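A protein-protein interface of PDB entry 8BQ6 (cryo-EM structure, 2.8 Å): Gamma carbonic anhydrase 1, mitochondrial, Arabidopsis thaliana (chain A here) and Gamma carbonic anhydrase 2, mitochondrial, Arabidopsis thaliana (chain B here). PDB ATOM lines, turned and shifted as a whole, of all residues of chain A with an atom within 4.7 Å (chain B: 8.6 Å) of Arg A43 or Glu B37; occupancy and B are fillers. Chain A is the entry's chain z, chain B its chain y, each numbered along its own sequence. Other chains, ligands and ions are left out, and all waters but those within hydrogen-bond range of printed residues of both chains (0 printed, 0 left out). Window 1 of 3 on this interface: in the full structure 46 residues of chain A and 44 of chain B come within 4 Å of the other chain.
The side-chain amide oxygen of Asn A47 sits at hydrogen-bond distance from the guanidinium group of Arg A43 (3.5 Å). The side-chain carboxylate of Glu B37 is in salt-bridge range of the guanidinium group of Arg B34, 2.8 Å away. The side-chain sulfur (SD) of Met A46 sits close to the guanidinium group (NH2) of Arg A43 (3.6 Å).
Among the printed residues, pairs that only touch across the chains: Arg A43 with Arg B34, Arg A43 with Glu B37, Leu A45 with Ile B35, Asn A47 with His B33 and Asn A47 with Arg B34.
Of chain A, only Arg A41 and Arg A43 come within 4 Å of Glu B37. Printed residues of chain A within 4 Å of Ile B35: Arg A43, Leu A45 and Asn A47. Of the printed residues of chain B, Arg A41 touches Glu B37. Ala A65 touches none of the printed residues of chain B.
OE2 of Glu B37 is in salt-bridge range of NE of Arg A41, at 3.2 Å. The guanidinium group (NH1) of Arg A43 lies within hydrogen-bond range of the backbone carbonyl oxygen (O) of Ile B35, at 3.0 Å. N of Ile B35 sits at hydrogen-bond distance from OD1 of Asn A47, 2.9 Å away.
Of the 8 printed residues of chain B, 4 touch a printed residue of chain A. Hydrophobic or aromatic side chains of chain A that line the printed part of chain B: Leu A45.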
ATOM      1  N   ARG A  41     -14.162   3.361  32.765  1.00  0.00           N
ATOM      2  CA  ARG A  41     -14.572   1.996  32.496  1.00  0.00           C
ATOM      3  C   ARG A  41     -14.746   1.741  31.008  1.00  0.00           C
ATOM      4  O   ARG A  41     -15.335   0.726  30.627  1.00  0.00           O
ATOM      5  CB  ARG A  41     -15.856   1.685  33.264  1.00  0.00           C
ATOM      6  CG  ARG A  41     -15.785   2.133  34.719  1.00  0.00           C
ATOM      7  CD  ARG A  41     -16.954   1.630  35.531  1.00  0.00           C
ATOM      8  NE  ARG A  41     -17.010   0.175  35.575  1.00  0.00           N
ATOM      9  CZ  ARG A  41     -17.819  -0.513  36.368  1.00  0.00           C
ATOM     10  NH1 ARG A  41     -18.646   0.092  37.202  1.00  0.00           N
ATOM     11  NH2 ARG A  41     -17.799  -1.842  36.320  1.00  0.00           N
ATOM     12  N   HIS A  42     -14.240   2.638  30.164  1.00  0.00           N
ATOM     13  CA  HIS A  42     -14.344   2.451  28.725  1.00  0.00           C
ATOM     14  C   HIS A  42     -13.551   1.230  28.289  1.00  0.00           C
ATOM     15  O   HIS A  42     -12.386   1.061  28.658  1.00  0.00           O
ATOM     16  CB  HIS A  42     -13.839   3.685  27.982  1.00  0.00           C
ATOM     17  CG  HIS A  42     -13.611   3.447  26.522  1.00  0.00           C
ATOM     18  ND1 HIS A  42     -14.643   3.393  25.609  1.00  0.00           N
ATOM     19  CD2 HIS A  42     -12.477   3.218  25.821  1.00  0.00           C
ATOM     20  CE1 HIS A  42     -14.151   3.159  24.406  1.00  0.00           C
ATOM     21  NE2 HIS A  42     -12.839   3.048  24.506  1.00  0.00           N
ATOM     22  N   ARG A  43     -14.190   0.382  27.493  1.00  0.00           N
ATOM     23  CA  ARG A  43     -13.546  -0.772  26.890  1.00  0.00           C
ATOM     24  C   ARG A  43     -13.539  -0.575  25.384  1.00  0.00           C
ATOM     25  O   ARG A  43     -14.580  -0.280  24.790  1.00  0.00           O
ATOM     26  CB  ARG A  43     -14.272  -2.067  27.257  1.00  0.00           C
ATOM     27  CG  ARG A  43     -13.983  -2.561  28.658  1.00  0.00           C
ATOM     28  CD  ARG A  43     -14.854  -3.742  29.023  1.00  0.00           C
ATOM     29  NE  ARG A  43     -16.257  -3.372  29.156  1.00  0.00           N
ATOM     30  CZ  ARG A  43     -17.255  -4.241  29.247  1.00  0.00           C
ATOM     31  NH1 ARG A  43     -17.038  -5.546  29.229  1.00  0.00           N
ATOM     32  NH2 ARG A  43     -18.500  -3.790  29.366  1.00  0.00           N
ATOM     33  N   THR A  44     -12.364  -0.721  24.775  1.00  0.00           N
ATOM     34  CA  THR A  44     -12.273  -0.623  23.324  1.00  0.00           C
ATOM     35  C   THR A  44     -13.120  -1.696  22.655  1.00  0.00           C
ATOM     36  O   THR A  44     -13.817  -1.428  21.669  1.00  0.00           O
ATOM     37  CB  THR A  44     -10.811  -0.734  22.895  1.00  0.00           C
ATOM     38  OG1 THR A  44     -10.023   0.174  23.673  1.00  0.00           O
ATOM     39  CG2 THR A  44     -10.655  -0.387  21.441  1.00  0.00           C
ATOM     40  N   LEU A  45     -13.082  -2.912  23.186  1.00  0.00           N
ATOM     41  CA  LEU A  45     -13.903  -4.016  22.720  1.00  0.00           C
ATOM     42  C   LEU A  45     -14.851  -4.416  23.838  1.00  0.00           C
ATOM     43  O   LEU A  45     -14.408  -4.854  24.904  1.00  0.00           O
ATOM     44  CB  LEU A  45     -13.033  -5.203  22.308  1.00  0.00           C
ATOM     45  CG  LEU A  45     -11.858  -4.849  21.399  1.00  0.00           C
ATOM     46  CD1 LEU A  45     -11.067  -6.096  21.072  1.00  0.00           C
ATOM     47  CD2 LEU A  45     -12.349  -4.179  20.130  1.00  0.00           C
ATOM     48  N   MET A  46     -16.146  -4.257  23.600  1.00  0.00           N
ATOM     49  CA  MET A  46     -17.148  -4.520  24.618  1.00  0.00           C
ATOM     50  C   MET A  46     -18.068  -5.631  24.149  1.00  0.00           C
ATOM     51  O   MET A  46     -18.531  -5.618  23.004  1.00  0.00           O
ATOM     52  CB  MET A  46     -17.961  -3.266  24.938  1.00  0.00           C
ATOM     53  CG  MET A  46     -18.788  -3.394  26.194  1.00  0.00           C
ATOM     54  SD  MET A  46     -19.818  -1.954  26.520  1.00  0.00           S
ATOM     55  CE  MET A  46     -21.262  -2.737  27.230  1.00  0.00           C
ATOM     56  N   ASN A  47     -18.334  -6.579  25.034  1.00  0.00           N
ATOM     57  CA  ASN A  47     -19.248  -7.668  24.750  1.00  0.00           C
ATOM     58  C   ASN A  47     -20.612  -7.390  25.368  1.00  0.00           C
ATOM     59  O   ASN A  47     -20.728  -6.685  26.375  1.00  0.00           O
ATOM     60  CB  ASN A  47     -18.678  -8.983  25.283  1.00  0.00           C
ATOM     61  CG  ASN A  47     -18.627  -9.024  26.793  1.00  0.00           C
ATOM     62  OD1 ASN A  47     -17.749  -8.425  27.410  1.00  0.00           O
ATOM     63  ND2 ASN A  47     -19.560  -9.745  27.397  1.00  0.00           N
ATOM     64  N   ALA A  65     -11.761   4.326  20.489  1.00  0.00           N
ATOM     65  CA  ALA A  65     -12.877   3.853  19.688  1.00  0.00           C
ATOM     66  C   ALA A  65     -13.716   2.852  20.478  1.00  0.00           C
ATOM     67  O   ALA A  65     -13.231   2.194  21.400  1.00  0.00           O
ATOM     68  CB  ALA A  65     -12.362   3.213  18.400  1.00  0.00           C
ATOM     69  N   HIS B  33     -16.541 -14.832  29.155  1.00  0.00           N
ATOM     70  CA  HIS B  33     -17.007 -14.056  28.014  1.00  0.00           C
ATOM     71  C   HIS B  33     -16.779 -12.564  28.191  1.00  0.00           C
ATOM     72  O   HIS B  33     -16.454 -11.875  27.219  1.00  0.00           O
ATOM     73  CB  HIS B  33     -18.490 -14.331  27.774  1.00  0.00           C
ATOM     74  CG  HIS B  33     -18.763 -15.688  27.210  1.00  0.00           C
ATOM     75  ND1 HIS B  33     -17.864 -16.347  26.400  1.00  0.00           N
ATOM     76  CD2 HIS B  33     -19.822 -16.518  27.352  1.00  0.00           C
ATOM     77  CE1 HIS B  33     -18.363 -17.522  26.059  1.00  0.00           C
ATOM     78  NE2 HIS B  33     -19.549 -17.651  26.624  1.00  0.00           N
ATOM     79  N   ARG B  34     -16.952 -12.071  29.423  1.00  0.00           N
ATOM     80  CA  ARG B  34     -16.833 -10.616  29.699  1.00  0.00           C
ATOM     81  C   ARG B  34     -15.405 -10.134  29.464  1.00  0.00           C
ATOM     82  O   ARG B  34     -14.473 -10.718  30.035  1.00  0.00           O
ATOM     83  CB  ARG B  34     -17.273 -10.269  31.123  1.00  0.00           C
ATOM     84  CG  ARG B  34     -17.917  -8.895  31.240  1.00  0.00           C
ATOM     85  CD  ARG B  34     -17.778  -8.294  32.622  1.00  0.00           C
ATOM     86  NE  ARG B  34     -18.281  -6.928  32.655  1.00  0.00           N
ATOM     87  CZ  ARG B  34     -17.522  -5.843  32.756  1.00  0.00           C
ATOM     88  NH1 ARG B  34     -16.206  -5.950  32.834  1.00  0.00           N
ATOM     89  NH2 ARG B  34     -18.086  -4.650  32.771  1.00  0.00           N
ATOM     90  N   ILE B  35     -15.262  -9.093  28.646  1.00  0.00           N
ATOM     91  CA  ILE B  35     -13.937  -8.524  28.455  1.00  0.00           C
ATOM     92  C   ILE B  35     -13.612  -7.624  29.639  1.00  0.00           C
ATOM     93  O   ILE B  35     -14.405  -6.753  30.016  1.00  0.00           O
ATOM     94  CB  ILE B  35     -13.871  -7.767  27.119  1.00  0.00           C
ATOM     95  CG1 ILE B  35     -13.964  -8.755  25.955  1.00  0.00           C
ATOM     96  CG2 ILE B  35     -12.582  -6.999  27.004  1.00  0.00           C
ATOM     97  CD1 ILE B  35     -14.233  -8.115  24.623  1.00  0.00           C
ATOM     98  N   GLU B  36     -12.451  -7.852  30.249  1.00  0.00           N
ATOM     99  CA  GLU B  36     -12.074  -7.145  31.465  1.00  0.00           C
ATOM    100  C   GLU B  36     -11.735  -5.688  31.173  1.00  0.00           C
ATOM    101  O   GLU B  36     -11.056  -5.374  30.193  1.00  0.00           O
ATOM    102  CB  GLU B  36     -10.880  -7.834  32.130  1.00  0.00           C
ATOM    103  CG  GLU B  36     -11.267  -8.982  33.058  1.00  0.00           C
ATOM    104  CD  GLU B  36     -10.069  -9.733  33.634  1.00  0.00           C
ATOM    105  OE1 GLU B  36      -8.934  -9.552  33.142  1.00  0.00           O
ATOM    106  OE2 GLU B  36     -10.267 -10.511  34.591  1.00  0.00           O
ATOM    107  N   GLU B  37     -12.227  -4.797  32.031  1.00  0.00           N
ATOM    108  CA  GLU B  37     -11.821  -3.403  31.966  1.00  0.00           C
ATOM    109  C   GLU B  37     -10.355  -3.281  32.353  1.00  0.00           C
ATOM    110  O   GLU B  37      -9.886  -3.911  33.303  1.00  0.00           O
ATOM    111  CB  GLU B  37     -12.678  -2.548  32.896  1.00  0.00           C
ATOM    112  CG  GLU B  37     -14.128  -2.449  32.484  1.00  0.00           C
ATOM    113  CD  GLU B  37     -15.051  -2.323  33.673  1.00  0.00           C
ATOM    114  OE1 GLU B  37     -16.226  -2.727  33.564  1.00  0.00           O
ATOM    115  OE2 GLU B  37     -14.602  -1.815  34.718  1.00  0.00           O
ATOM    116  N   HIS B  38      -9.627  -2.457  31.610  1.00  0.00           N
ATOM    117  CA  HIS B  38      -8.196  -2.328  31.818  1.00  0.00           C
ATOM    118  C   HIS B  38      -7.851  -0.870  32.076  1.00  0.00           C
ATOM    119  O   HIS B  38      -8.700   0.021  31.997  1.00  0.00           O
ATOM    120  CB  HIS B  38      -7.414  -2.877  30.620  1.00  0.00           C
ATOM    121  CG  HIS B  38      -7.209  -4.360  30.660  1.00  0.00           C
ATOM    122  ND1 HIS B  38      -7.569  -5.132  31.744  1.00  0.00           N
ATOM    123  CD2 HIS B  38      -6.669  -5.210  29.755  1.00  0.00           C
ATOM    124  CE1 HIS B  38      -7.262  -6.394  31.504  1.00  0.00           C
ATOM    125  NE2 HIS B  38      -6.715  -6.469  30.304  1.00  0.00           N
ATOM    126  N   LEU B  39      -6.582  -0.642  32.404  1.00  0.00           N
ATOM    127  CA  LEU B  39      -6.068   0.711  32.546  1.00  0.00           C
ATOM    128  C   LEU B  39      -6.223   1.472  31.236  1.00  0.00           C
ATOM    129  O   LEU B  39      -6.260   0.879  30.155  1.00  0.00           O
ATOM    130  CB  LEU B  39      -4.598   0.663  32.947  1.00  0.00           C
ATOM    131  CG  LEU B  39      -3.981   1.821  33.722  1.00  0.00           C
ATOM    132  CD1 LEU B  39      -4.707   2.072  35.021  1.00  0.00           C
ATOM    133  CD2 LEU B  39      -2.520   1.517  33.962  1.00  0.00           C
ATOM    134  N   SER B  40      -6.305   2.795  31.335  1.00  0.00           N
ATOM    135  CA  SER B  40      -6.567   3.614  30.160  1.00  0.00           C
ATOM    136  C   SER B  40      -5.321   3.732  29.294  1.00  0.00           C
ATOM    137  O   SER B  40      -4.246   4.100  29.775  1.00  0.00           O
ATOM    138  CB  SER B  40      -7.048   5.000  30.578  1.00  0.00           C
ATOM    139  OG  SER B  40      -7.759   5.626  29.526  1.00  0.00           O
